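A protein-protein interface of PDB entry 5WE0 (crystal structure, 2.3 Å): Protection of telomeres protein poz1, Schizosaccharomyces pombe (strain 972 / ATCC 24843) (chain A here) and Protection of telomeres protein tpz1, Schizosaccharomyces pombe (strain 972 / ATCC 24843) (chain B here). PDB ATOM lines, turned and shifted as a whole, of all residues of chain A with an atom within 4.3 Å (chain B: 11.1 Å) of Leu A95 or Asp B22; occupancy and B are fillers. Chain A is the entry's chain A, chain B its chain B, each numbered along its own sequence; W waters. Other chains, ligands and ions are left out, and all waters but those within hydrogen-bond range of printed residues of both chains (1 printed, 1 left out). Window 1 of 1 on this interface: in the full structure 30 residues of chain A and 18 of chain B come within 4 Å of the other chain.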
ATOM      1  N   PHE A  60       5.763 -31.698   0.676  1.00  0.00           N
ATOM      2  CA  PHE A  60       5.094 -30.452   0.322  1.00  0.00           C
ATOM      3  C   PHE A  60       4.300 -30.613  -0.962  1.00  0.00           C
ATOM      4  O   PHE A  60       3.132 -30.226  -1.033  1.00  0.00           O
ATOM      5  CB  PHE A  60       6.086 -29.305   0.156  1.00  0.00           C
ATOM      6  CG  PHE A  60       5.423 -28.074  -0.369  1.00  0.00           C
ATOM      7  CD1 PHE A  60       4.654 -27.279   0.470  1.00  0.00           C
ATOM      8  CD2 PHE A  60       5.465 -27.769  -1.729  1.00  0.00           C
ATOM      9  CE1 PHE A  60       3.997 -26.170  -0.028  1.00  0.00           C
ATOM     10  CE2 PHE A  60       4.802 -26.670  -2.226  1.00  0.00           C
ATOM     11  CZ  PHE A  60       4.066 -25.872  -1.380  1.00  0.00           C
ATOM     12  N   LEU A  90      -4.893 -24.695  -3.724  1.00  0.00           N
ATOM     13  CA  LEU A  90      -4.843 -23.244  -3.591  1.00  0.00           C
ATOM     14  C   LEU A  90      -4.015 -22.681  -4.748  1.00  0.00           C
ATOM     15  O   LEU A  90      -2.780 -22.673  -4.702  1.00  0.00           O
ATOM     16  CB  LEU A  90      -4.254 -22.858  -2.236  1.00  0.00           C
ATOM     17  CG  LEU A  90      -4.065 -21.346  -2.014  1.00  0.00           C
ATOM     18  CD1 LEU A  90      -5.395 -20.571  -2.189  1.00  0.00           C
ATOM     19  CD2 LEU A  90      -3.430 -21.043  -0.668  1.00  0.00           C
ATOM     20  N   GLU A  92      -2.617 -19.922  -5.854  1.00  0.00           N
ATOM     21  CA  GLU A  92      -2.173 -18.585  -5.520  1.00  0.00           C
ATOM     22  C   GLU A  92      -0.766 -18.468  -6.092  1.00  0.00           C
ATOM     23  O   GLU A  92       0.038 -19.400  -5.965  1.00  0.00           O
ATOM     24  CB  GLU A  92      -2.215 -18.350  -3.991  1.00  0.00           C
ATOM     25  CG  GLU A  92      -1.918 -16.902  -3.573  1.00  0.00           C
ATOM     26  CD  GLU A  92      -0.437 -16.587  -3.354  1.00  0.00           C
ATOM     27  OE1 GLU A  92       0.233 -17.344  -2.602  1.00  0.00           O
ATOM     28  OE2 GLU A  92       0.062 -15.585  -3.961  1.00  0.00           O
ATOM     29  N   TYR A  93      -0.496 -17.349  -6.766  1.00  0.00           N
ATOM     30  CA  TYR A  93       0.730 -17.194  -7.554  1.00  0.00           C
ATOM     31  C   TYR A  93       1.978 -17.520  -6.739  1.00  0.00           C
ATOM     32  O   TYR A  93       2.849 -18.282  -7.184  1.00  0.00           O
ATOM     33  CB  TYR A  93       0.811 -15.764  -8.096  1.00  0.00           C
ATOM     34  CG  TYR A  93       2.204 -15.318  -8.321  1.00  0.00           C
ATOM     35  CD1 TYR A  93       2.989 -15.921  -9.327  1.00  0.00           C
ATOM     36  CD2 TYR A  93       2.781 -14.332  -7.507  1.00  0.00           C
ATOM     37  CE1 TYR A  93       4.309 -15.547  -9.532  1.00  0.00           C
ATOM     38  CE2 TYR A  93       4.113 -13.949  -7.703  1.00  0.00           C
ATOM     39  CZ  TYR A  93       4.869 -14.566  -8.725  1.00  0.00           C
ATOM     40  OH  TYR A  93       6.181 -14.216  -8.951  1.00  0.00           O
ATOM     41  N   SER A  94       2.084 -16.938  -5.541  1.00  0.00           N
ATOM     42  CA  SER A  94       3.296 -17.082  -4.747  1.00  0.00           C
ATOM     43  C   SER A  94       3.503 -18.535  -4.317  1.00  0.00           C
ATOM     44  O   SER A  94       4.605 -19.084  -4.459  1.00  0.00           O
ATOM     45  CB  SER A  94       3.227 -16.150  -3.539  1.00  0.00           C
ATOM     46  OG  SER A  94       4.390 -16.265  -2.742  1.00  0.00           O
ATOM     47  N   LEU A  95       2.437 -19.185  -3.830  1.00  0.00           N
ATOM     48  CA  LEU A  95       2.522 -20.579  -3.408  1.00  0.00           C
ATOM     49  C   LEU A  95       2.896 -21.487  -4.574  1.00  0.00           C
ATOM     50  O   LEU A  95       3.788 -22.335  -4.450  1.00  0.00           O
ATOM     51  CB  LEU A  95       1.193 -21.021  -2.787  1.00  0.00           C
ATOM     52  CG  LEU A  95       0.989 -22.512  -2.491  1.00  0.00           C
ATOM     53  CD1 LEU A  95       1.890 -22.989  -1.357  1.00  0.00           C
ATOM     54  CD2 LEU A  95      -0.480 -22.838  -2.194  1.00  0.00           C
ATOM     55  N   ILE A  96       2.206 -21.339  -5.713  1.00  0.00           N
ATOM     56  CA  ILE A  96       2.451 -22.227  -6.847  1.00  0.00           C
ATOM     57  C   ILE A  96       3.848 -21.999  -7.421  1.00  0.00           C
ATOM     58  O   ILE A  96       4.516 -22.936  -7.860  1.00  0.00           O
ATOM     59  CB  ILE A  96       1.362 -22.035  -7.919  1.00  0.00           C
ATOM     60  CG1 ILE A  96      -0.025 -22.439  -7.381  1.00  0.00           C
ATOM     61  CG2 ILE A  96       1.725 -22.839  -9.171  1.00  0.00           C
ATOM     62  CD1 ILE A  96      -0.098 -23.890  -6.824  1.00  0.00           C
ATOM     63  N   SER A  97       4.319 -20.768  -7.412  1.00  0.00           N
ATOM     64  CA  SER A  97       5.685 -20.506  -7.843  1.00  0.00           C
ATOM     65  C   SER A  97       6.692 -21.218  -6.937  1.00  0.00           C
ATOM     66  O   SER A  97       7.682 -21.783  -7.423  1.00  0.00           O
ATOM     67  CB  SER A  97       5.914 -18.993  -7.870  1.00  0.00           C
ATOM     68  OG  SER A  97       7.072 -18.656  -8.584  1.00  0.00           O
ATOM     69  N   ASN A  98       6.462 -21.195  -5.613  1.00  0.00           N
ATOM     70  CA  ASN A  98       7.330 -21.924  -4.691  1.00  0.00           C
ATOM     71  C   ASN A  98       7.244 -23.424  -4.922  1.00  0.00           C
ATOM     72  O   ASN A  98       8.265 -24.126  -4.901  1.00  0.00           O
ATOM     73  CB  ASN A  98       6.968 -21.603  -3.245  1.00  0.00           C
ATOM     74  CG  ASN A  98       7.301 -20.164  -2.860  1.00  0.00           C
ATOM     75  OD1 ASN A  98       8.037 -19.477  -3.557  1.00  0.00           O
ATOM     76  ND2 ASN A  98       6.747 -19.708  -1.744  1.00  0.00           N
ATOM     77  N   ALA A  99       6.029 -23.930  -5.153  1.00  0.00           N
ATOM     78  CA  ALA A  99       5.861 -25.350  -5.424  1.00  0.00           C
ATOM     79  C   ALA A  99       6.646 -25.773  -6.666  1.00  0.00           C
ATOM     80  O   ALA A  99       7.204 -26.875  -6.702  1.00  0.00           O
ATOM     81  CB  ALA A  99       4.376 -25.674  -5.581  1.00  0.00           C
ATOM     82  N   ARG A 102      10.212 -26.045  -5.828  1.00  0.00           N
ATOM     83  CA  ARG A 102      10.399 -27.248  -5.034  1.00  0.00           C
ATOM     84  C   ARG A 102      10.417 -28.469  -5.952  1.00  0.00           C
ATOM     85  O   ARG A 102      11.264 -29.351  -5.803  1.00  0.00           O
ATOM     86  CB  ARG A 102       9.287 -27.386  -3.993  1.00  0.00           C
ATOM     87  CG  ARG A 102       9.448 -26.471  -2.789  1.00  0.00           C
ATOM     88  CD  ARG A 102       8.395 -26.760  -1.731  1.00  0.00           C
ATOM     89  NE  ARG A 102       7.847 -25.535  -1.156  1.00  0.00           N
ATOM     90  CZ  ARG A 102       8.533 -24.698  -0.385  1.00  0.00           C
ATOM     91  NH1 ARG A 102       9.801 -24.952  -0.093  1.00  0.00           N
ATOM     92  NH2 ARG A 102       7.953 -23.606   0.094  1.00  0.00           N
ATOM     93  N   GLY B  14      14.672 -18.080   4.303  1.00  0.00           N
ATOM     94  CA  GLY B  14      15.216 -19.339   3.837  1.00  0.00           C
ATOM     95  C   GLY B  14      14.143 -20.378   3.576  1.00  0.00           C
ATOM     96  O   GLY B  14      12.946 -20.176   3.808  1.00  0.00           O
ATOM     97  N   SER B  15      14.600 -21.548   3.128  1.00  0.00           N
ATOM     98  CA  SER B  15      13.670 -22.559   2.624  1.00  0.00           C
ATOM     99  C   SER B  15      12.729 -23.069   3.705  1.00  0.00           C
ATOM    100  O   SER B  15      11.576 -23.404   3.411  1.00  0.00           O
ATOM    101  CB  SER B  15      14.436 -23.724   2.011  1.00  0.00           C
ATOM    102  OG  SER B  15      15.498 -23.237   1.232  1.00  0.00           O
ATOM    103  N   PHE B  16      13.207 -23.186   4.947  1.00  0.00           N
ATOM    104  CA  PHE B  16      12.352 -23.711   6.009  1.00  0.00           C
ATOM    105  C   PHE B  16      11.288 -22.708   6.396  1.00  0.00           C
ATOM    106  O   PHE B  16      10.148 -23.089   6.676  1.00  0.00           O
ATOM    107  CB  PHE B  16      13.195 -24.109   7.223  1.00  0.00           C
ATOM    108  CG  PHE B  16      14.051 -25.297   6.964  1.00  0.00           C
ATOM    109  CD1 PHE B  16      13.528 -26.581   7.096  1.00  0.00           C
ATOM    110  CD2 PHE B  16      15.331 -25.146   6.502  1.00  0.00           C
ATOM    111  CE1 PHE B  16      14.293 -27.693   6.803  1.00  0.00           C
ATOM    112  CE2 PHE B  16      16.104 -26.263   6.220  1.00  0.00           C
ATOM    113  CZ  PHE B  16      15.579 -27.530   6.384  1.00  0.00           C
ATOM    114  N   PHE B  17      11.634 -21.419   6.415  1.00  0.00           N
ATOM    115  CA  PHE B  17      10.623 -20.405   6.674  1.00  0.00           C
ATOM    116  C   PHE B  17       9.601 -20.344   5.541  1.00  0.00           C
ATOM    117  O   PHE B  17       8.392 -20.284   5.798  1.00  0.00           O
ATOM    118  CB  PHE B  17      11.284 -19.044   6.902  1.00  0.00           C
ATOM    119  CG  PHE B  17      10.298 -17.929   7.178  1.00  0.00           C
ATOM    120  CD1 PHE B  17       9.462 -17.982   8.294  1.00  0.00           C
ATOM    121  CD2 PHE B  17      10.226 -16.822   6.342  1.00  0.00           C
ATOM    122  CE1 PHE B  17       8.544 -16.962   8.555  1.00  0.00           C
ATOM    123  CE2 PHE B  17       9.318 -15.793   6.603  1.00  0.00           C
ATOM    124  CZ  PHE B  17       8.475 -15.865   7.707  1.00  0.00           C
ATOM    125  N   GLU B  18      10.064 -20.387   4.283  1.00  0.00           N
ATOM    126  CA  GLU B  18       9.134 -20.349   3.152  1.00  0.00           C
ATOM    127  C   GLU B  18       8.234 -21.576   3.142  1.00  0.00           C
ATOM    128  O   GLU B  18       7.030 -21.470   2.869  1.00  0.00           O
ATOM    129  CB  GLU B  18       9.888 -20.238   1.823  1.00  0.00           C
ATOM    130  CG  GLU B  18      10.788 -19.025   1.680  1.00  0.00           C
ATOM    131  CD  GLU B  18      10.070 -17.697   1.966  1.00  0.00           C
ATOM    132  OE1 GLU B  18       8.839 -17.598   1.725  1.00  0.00           O
ATOM    133  OE2 GLU B  18      10.739 -16.744   2.437  1.00  0.00           O
ATOM    134  N   LEU B  19       8.788 -22.747   3.470  1.00  0.00           N
ATOM    135  CA  LEU B  19       7.949 -23.939   3.552  1.00  0.00           C
ATOM    136  C   LEU B  19       6.893 -23.783   4.644  1.00  0.00           C
ATOM    137  O   LEU B  19       5.715 -24.111   4.439  1.00  0.00           O
ATOM    138  CB  LEU B  19       8.808 -25.187   3.804  1.00  0.00           C
ATOM    139  CG  LEU B  19       7.920 -26.427   3.918  1.00  0.00           C
ATOM    140  CD1 LEU B  19       7.397 -26.790   2.548  1.00  0.00           C
ATOM    141  CD2 LEU B  19       8.606 -27.604   4.570  1.00  0.00           C
ATOM    142  N   LEU B  20       7.292 -23.251   5.801  1.00  0.00           N
ATOM    143  CA  LEU B  20       6.348 -23.033   6.897  1.00  0.00           C
ATOM    144  C   LEU B  20       5.171 -22.166   6.464  1.00  0.00           C
ATOM    145  O   LEU B  20       4.005 -22.535   6.665  1.00  0.00           O
ATOM    146  CB  LEU B  20       7.077 -22.399   8.084  1.00  0.00           C
ATOM    147  CG  LEU B  20       6.255 -21.740   9.191  1.00  0.00           C
ATOM    148  CD1 LEU B  20       5.381 -22.753   9.877  1.00  0.00           C
ATOM    149  CD2 LEU B  20       7.188 -21.026  10.189  1.00  0.00           C
ATOM    150  N   ARG B  21       5.451 -21.006   5.858  1.00  0.00           N
ATOM    151  CA  ARG B  21       4.361 -20.111   5.472  1.00  0.00           C
ATOM    152  C   ARG B  21       3.460 -20.748   4.422  1.00  0.00           C
ATOM    153  O   ARG B  21       2.231 -20.628   4.493  1.00  0.00           O
ATOM    154  CB  ARG B  21       4.898 -18.774   4.973  1.00  0.00           C
ATOM    155  CG  ARG B  21       5.499 -17.951   6.070  1.00  0.00           C
ATOM    156  CD  ARG B  21       5.764 -16.512   5.611  1.00  0.00           C
ATOM    157  NE  ARG B  21       6.387 -16.454   4.298  1.00  0.00           N
ATOM    158  CZ  ARG B  21       6.810 -15.328   3.745  1.00  0.00           C
ATOM    159  NH1 ARG B  21       6.680 -14.184   4.407  1.00  0.00           N
ATOM    160  NH2 ARG B  21       7.380 -15.358   2.552  1.00  0.00           N
ATOM    161  N   ASP B  22       4.052 -21.432   3.439  1.00  0.00           N
ATOM    162  CA  ASP B  22       3.258 -22.092   2.403  1.00  0.00           C
ATOM    163  C   ASP B  22       2.404 -23.203   2.985  1.00  0.00           C
ATOM    164  O   ASP B  22       1.272 -23.424   2.538  1.00  0.00           O
ATOM    165  CB  ASP B  22       4.172 -22.663   1.319  1.00  0.00           C
ATOM    166  CG  ASP B  22       4.888 -21.582   0.533  1.00  0.00           C
ATOM    167  OD1 ASP B  22       4.486 -20.385   0.628  1.00  0.00           O
ATOM    168  OD2 ASP B  22       5.844 -21.942  -0.195  1.00  0.00           O
ATOM    169  N   TRP B  23       2.970 -23.963   3.925  1.00  0.00           N
ATOM    170  CA  TRP B  23       2.234 -25.017   4.609  1.00  0.00           C
ATOM    171  C   TRP B  23       1.027 -24.457   5.336  1.00  0.00           C
ATOM    172  O   TRP B  23      -0.060 -25.049   5.305  1.00  0.00           O
ATOM    173  CB  TRP B  23       3.160 -25.725   5.595  1.00  0.00           C
ATOM    174  CG  TRP B  23       2.702 -27.069   5.974  1.00  0.00           C
ATOM    175  CD1 TRP B  23       1.771 -27.389   6.925  1.00  0.00           C
ATOM    176  CD2 TRP B  23       3.153 -28.306   5.413  1.00  0.00           C
ATOM    177  NE1 TRP B  23       1.623 -28.759   6.994  1.00  0.00           N
ATOM    178  CE2 TRP B  23       2.459 -29.344   6.075  1.00  0.00           C
ATOM    179  CE3 TRP B  23       4.090 -28.635   4.428  1.00  0.00           C
ATOM    180  CZ2 TRP B  23       2.659 -30.691   5.772  1.00  0.00           C
ATOM    181  CZ3 TRP B  23       4.291 -29.984   4.125  1.00  0.00           C
ATOM    182  CH2 TRP B  23       3.575 -30.991   4.794  1.00  0.00           C
ATOM    183  N   LYS B  24       1.210 -23.326   6.019  1.00  0.00           N
ATOM    184  CA  LYS B  24       0.094 -22.670   6.699  1.00  0.00           C
ATOM    185  C   LYS B  24      -0.977 -22.231   5.697  1.00  0.00           C
ATOM    186  O   LYS B  24      -2.153 -22.563   5.866  1.00  0.00           O
ATOM    187  CB  LYS B  24       0.632 -21.494   7.523  1.00  0.00           C
ATOM    188  CG  LYS B  24       1.547 -21.964   8.673  1.00  0.00           C
ATOM    189  CD  LYS B  24       2.069 -20.841   9.586  1.00  0.00           C
ATOM    190  CE  LYS B  24       1.027 -20.317  10.562  1.00  0.00           C
ATOM    191  NZ  LYS B  24       0.110 -19.331   9.924  1.00  0.00           N
ATOM    192  N   LYS B  25      -0.585 -21.604   4.582  1.00  0.00           N
ATOM    193  CA  LYS B  25      -1.585 -21.226   3.574  1.00  0.00           C
ATOM    194  C   LYS B  25      -2.435 -22.424   3.134  1.00  0.00           C
ATOM    195  O   LYS B  25      -3.659 -22.309   2.984  1.00  0.00           O
ATOM    196  CB  LYS B  25      -0.909 -20.593   2.366  1.00  0.00           C
ATOM    197  CG  LYS B  25      -0.331 -19.221   2.616  1.00  0.00           C
ATOM    198  CD  LYS B  25       0.179 -18.690   1.285  1.00  0.00           C
ATOM    199  CE  LYS B  25       1.048 -17.467   1.461  1.00  0.00           C
ATOM    200  NZ  LYS B  25       1.773 -17.183   0.189  1.00  0.00           N
ATOM    201  N   ILE B  26      -1.799 -23.568   2.866  1.00  0.00           N
ATOM    202  CA  ILE B  26      -2.542 -24.748   2.417  1.00  0.00           C
ATOM    203  C   ILE B  26      -3.514 -25.231   3.492  1.00  0.00           C
ATOM    204  O   ILE B  26      -4.656 -25.589   3.190  1.00  0.00           O
ATOM    205  CB  ILE B  26      -1.577 -25.878   2.001  1.00  0.00           C
ATOM    206  CG1 ILE B  26      -0.702 -25.473   0.805  1.00  0.00           C
ATOM    207  CG2 ILE B  26      -2.354 -27.153   1.688  1.00  0.00           C
ATOM    208  CD1 ILE B  26       0.511 -26.396   0.657  1.00  0.00           C
ATOM    209  N   GLU B  27      -3.063 -25.307   4.749  1.00  0.00           N
ATOM    210  CA  GLU B  27      -3.910 -25.854   5.810  1.00  0.00           C
ATOM    211  C   GLU B  27      -5.122 -24.964   6.071  1.00  0.00           C
ATOM    212  O   GLU B  27      -6.257 -25.438   6.196  1.00  0.00           O
ATOM    213  CB  GLU B  27      -3.087 -26.016   7.084  1.00  0.00           C
ATOM    214  CG  GLU B  27      -3.855 -26.727   8.195  1.00  0.00           C
ATOM    215  CD  GLU B  27      -2.964 -27.154   9.359  1.00  0.00           C
ATOM    216  OE1 GLU B  27      -1.848 -26.590   9.509  1.00  0.00           O
ATOM    217  OE2 GLU B  27      -3.384 -28.077  10.103  1.00  0.00           O
ATOM    218  N   GLU B  28      -4.876 -23.658   6.096  1.00  0.00           N
ATOM    219  CA  GLU B  28      -5.936 -22.683   6.303  1.00  0.00           C
ATOM    220  C   GLU B  28      -6.969 -22.793   5.184  1.00  0.00           C
ATOM    221  O   GLU B  28      -8.172 -22.815   5.442  1.00  0.00           O
ATOM    222  CB  GLU B  28      -5.363 -21.266   6.354  1.00  0.00           C
ATOM    223  CG  GLU B  28      -4.099 -21.138   7.188  1.00  0.00           C
ATOM    224  CD  GLU B  28      -4.216 -20.077   8.265  1.00  0.00           C
ATOM    225  OE1 GLU B  28      -5.103 -19.205   8.148  1.00  0.00           O
ATOM    226  OE2 GLU B  28      -3.422 -20.115   9.228  1.00  0.00           O
ATOM    227  N   PHE B  29      -6.496 -22.864   3.941  1.00  0.00           N
ATOM    228  CA  PHE B  29      -7.395 -22.984   2.798  1.00  0.00           C
ATOM    229  C   PHE B  29      -8.256 -24.238   2.867  1.00  0.00           C
ATOM    230  O   PHE B  29      -9.451 -24.188   2.557  1.00  0.00           O
ATOM    231  CB  PHE B  29      -6.578 -22.983   1.500  1.00  0.00           C
ATOM    232  CG  PHE B  29      -7.419 -23.113   0.268  1.00  0.00           C
ATOM    233  CD1 PHE B  29      -8.165 -22.033  -0.180  1.00  0.00           C
ATOM    234  CD2 PHE B  29      -7.508 -24.310  -0.407  1.00  0.00           C
ATOM    235  CE1 PHE B  29      -8.956 -22.145  -1.291  1.00  0.00           C
ATOM    236  CE2 PHE B  29      -8.301 -24.419  -1.537  1.00  0.00           C
ATOM    237  CZ  PHE B  29      -9.024 -23.344  -1.972  1.00  0.00           C
ATOM    238  N   ARG B  30      -7.673 -25.376   3.273  1.00  0.00           N
ATOM    239  CA  ARG B  30      -8.427 -26.630   3.324  1.00  0.00           C
ATOM    240  C   ARG B  30      -9.415 -26.701   4.488  1.00  0.00           C
ATOM    241  O   ARG B  30     -10.238 -27.629   4.513  1.00  0.00           O
ATOM    242  CB  ARG B  30      -7.507 -27.854   3.428  1.00  0.00           C
ATOM    243  CG  ARG B  30      -6.398 -27.959   2.387  1.00  0.00           C
ATOM    244  CD  ARG B  30      -6.614 -29.140   1.446  1.00  0.00           C
ATOM    245  NE  ARG B  30      -5.813 -28.980   0.236  1.00  0.00           N
ATOM    246  CZ  ARG B  30      -4.651 -29.588   0.010  1.00  0.00           C
ATOM    247  NH1 ARG B  30      -4.150 -30.437   0.900  1.00  0.00           N
ATOM    248  NH2 ARG B  30      -3.996 -29.353  -1.116  1.00  0.00           N
HETATM  249  O   HOH W   1       4.010 -18.194  -0.744  1.00  0.00           O
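The backbone NH (N) of Ser A94 is in hydrogen-bond range of the side-chain carboxylate (OE2) of Glu A92.
OE1 of Glu A92 lies within hydrogen-bond range of N of Leu A95 (3.1 Å).
The side-chain carboxylate (OE1) of Glu B18 lies within salt-bridge range of the guanidinium group (NH2) of Arg B21 (2.8 Å).
Water W1 lies within hydrogen-bond range of NZ of Lys B25 (2.6 Å), OD1 of Asp B22 (2.6 Å), OG of Ser A94 (2.8 Å) and ND2 of Asn A98 (3.3 Å).
Hydrophobic or aromatic side chains of chain A within 4 Å of the printed part of chain B: Phe A60, Leu A90 and Leu A95.
Along chain A the printed residues that touch a printed residue of chain B span positions 60 to 102.
Along chain B the printed residues that touch a printed residue of chain A span positions 18 to 29.
Among the printed residues, 13 pairs touch across the chains.
Among the printed residues, Asp or Glu carboxylates within 4 Å of a Lys or Arg side-chain nitrogen of the other chain: Glu A92 with Lys B25 (3.2 Å) and Arg A102 with Asp B22 (2.7 Å).
Of chain B, only Lys B25 (3.9 Å) and Phe B29 (3.7 Å) come within 4 Å of Leu A90.
Glu A92 touches just one residue of chain B: Lys B25.
Of the printed residues of chain B, Leu A95 touches Asp B22 (3.5 Å) and Ile B26 (3.998 Å).
No residue of chain B comes within 4 Å of Ile A96.
Printed residues of chain A within 4 Å of Leu B19: Phe A60 and Arg A102.
Asp B22 touches just these residues of chain A: Phe A60, Leu A95, Asn A98 and Arg A102.
Of the printed residues of chain A, Trp B23 touches Phe A60.
Of the printed residues of chain A, Lys B25 touches Leu A90 and Glu A92.
The nearest printed residue of chain A that does not touch Asp B22 is Ser A94 (5.3 Å).
The side-chain carboxylate (OE1) of Glu A92 lies within salt-bridge range of the side-chain amino group (NZ) of Lys B25, 3.2 Å away.
The side-chain amide nitrogen (ND2) of Asn A98 is in hydrogen-bond range of the side-chain carboxylate (OD2) of Asp B22.
OD2 of Asp B22 is in salt-bridge range of NH2 of Arg A102, at 2.7 Å.
Among the printed residues, merely in contact across the chains: Phe A60 with Leu B19 (3.5 Å), Phe A60 with Asp B22 (3.8 Å), Phe A60 with Trp B23 (3.9 Å), Phe A60 with Ile B26 (3.6 Å), Leu A90 with Lys B25 (3.9 Å), Leu A90 with Phe B29 (3.7 Å), Leu A95 with Asp B22 (3.5 Å), Leu A95 with Ile B26 (3.998 Å), Arg A102 with Glu B18 (3.6 Å) and Arg A102 with Leu B19 (3.5 Å).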
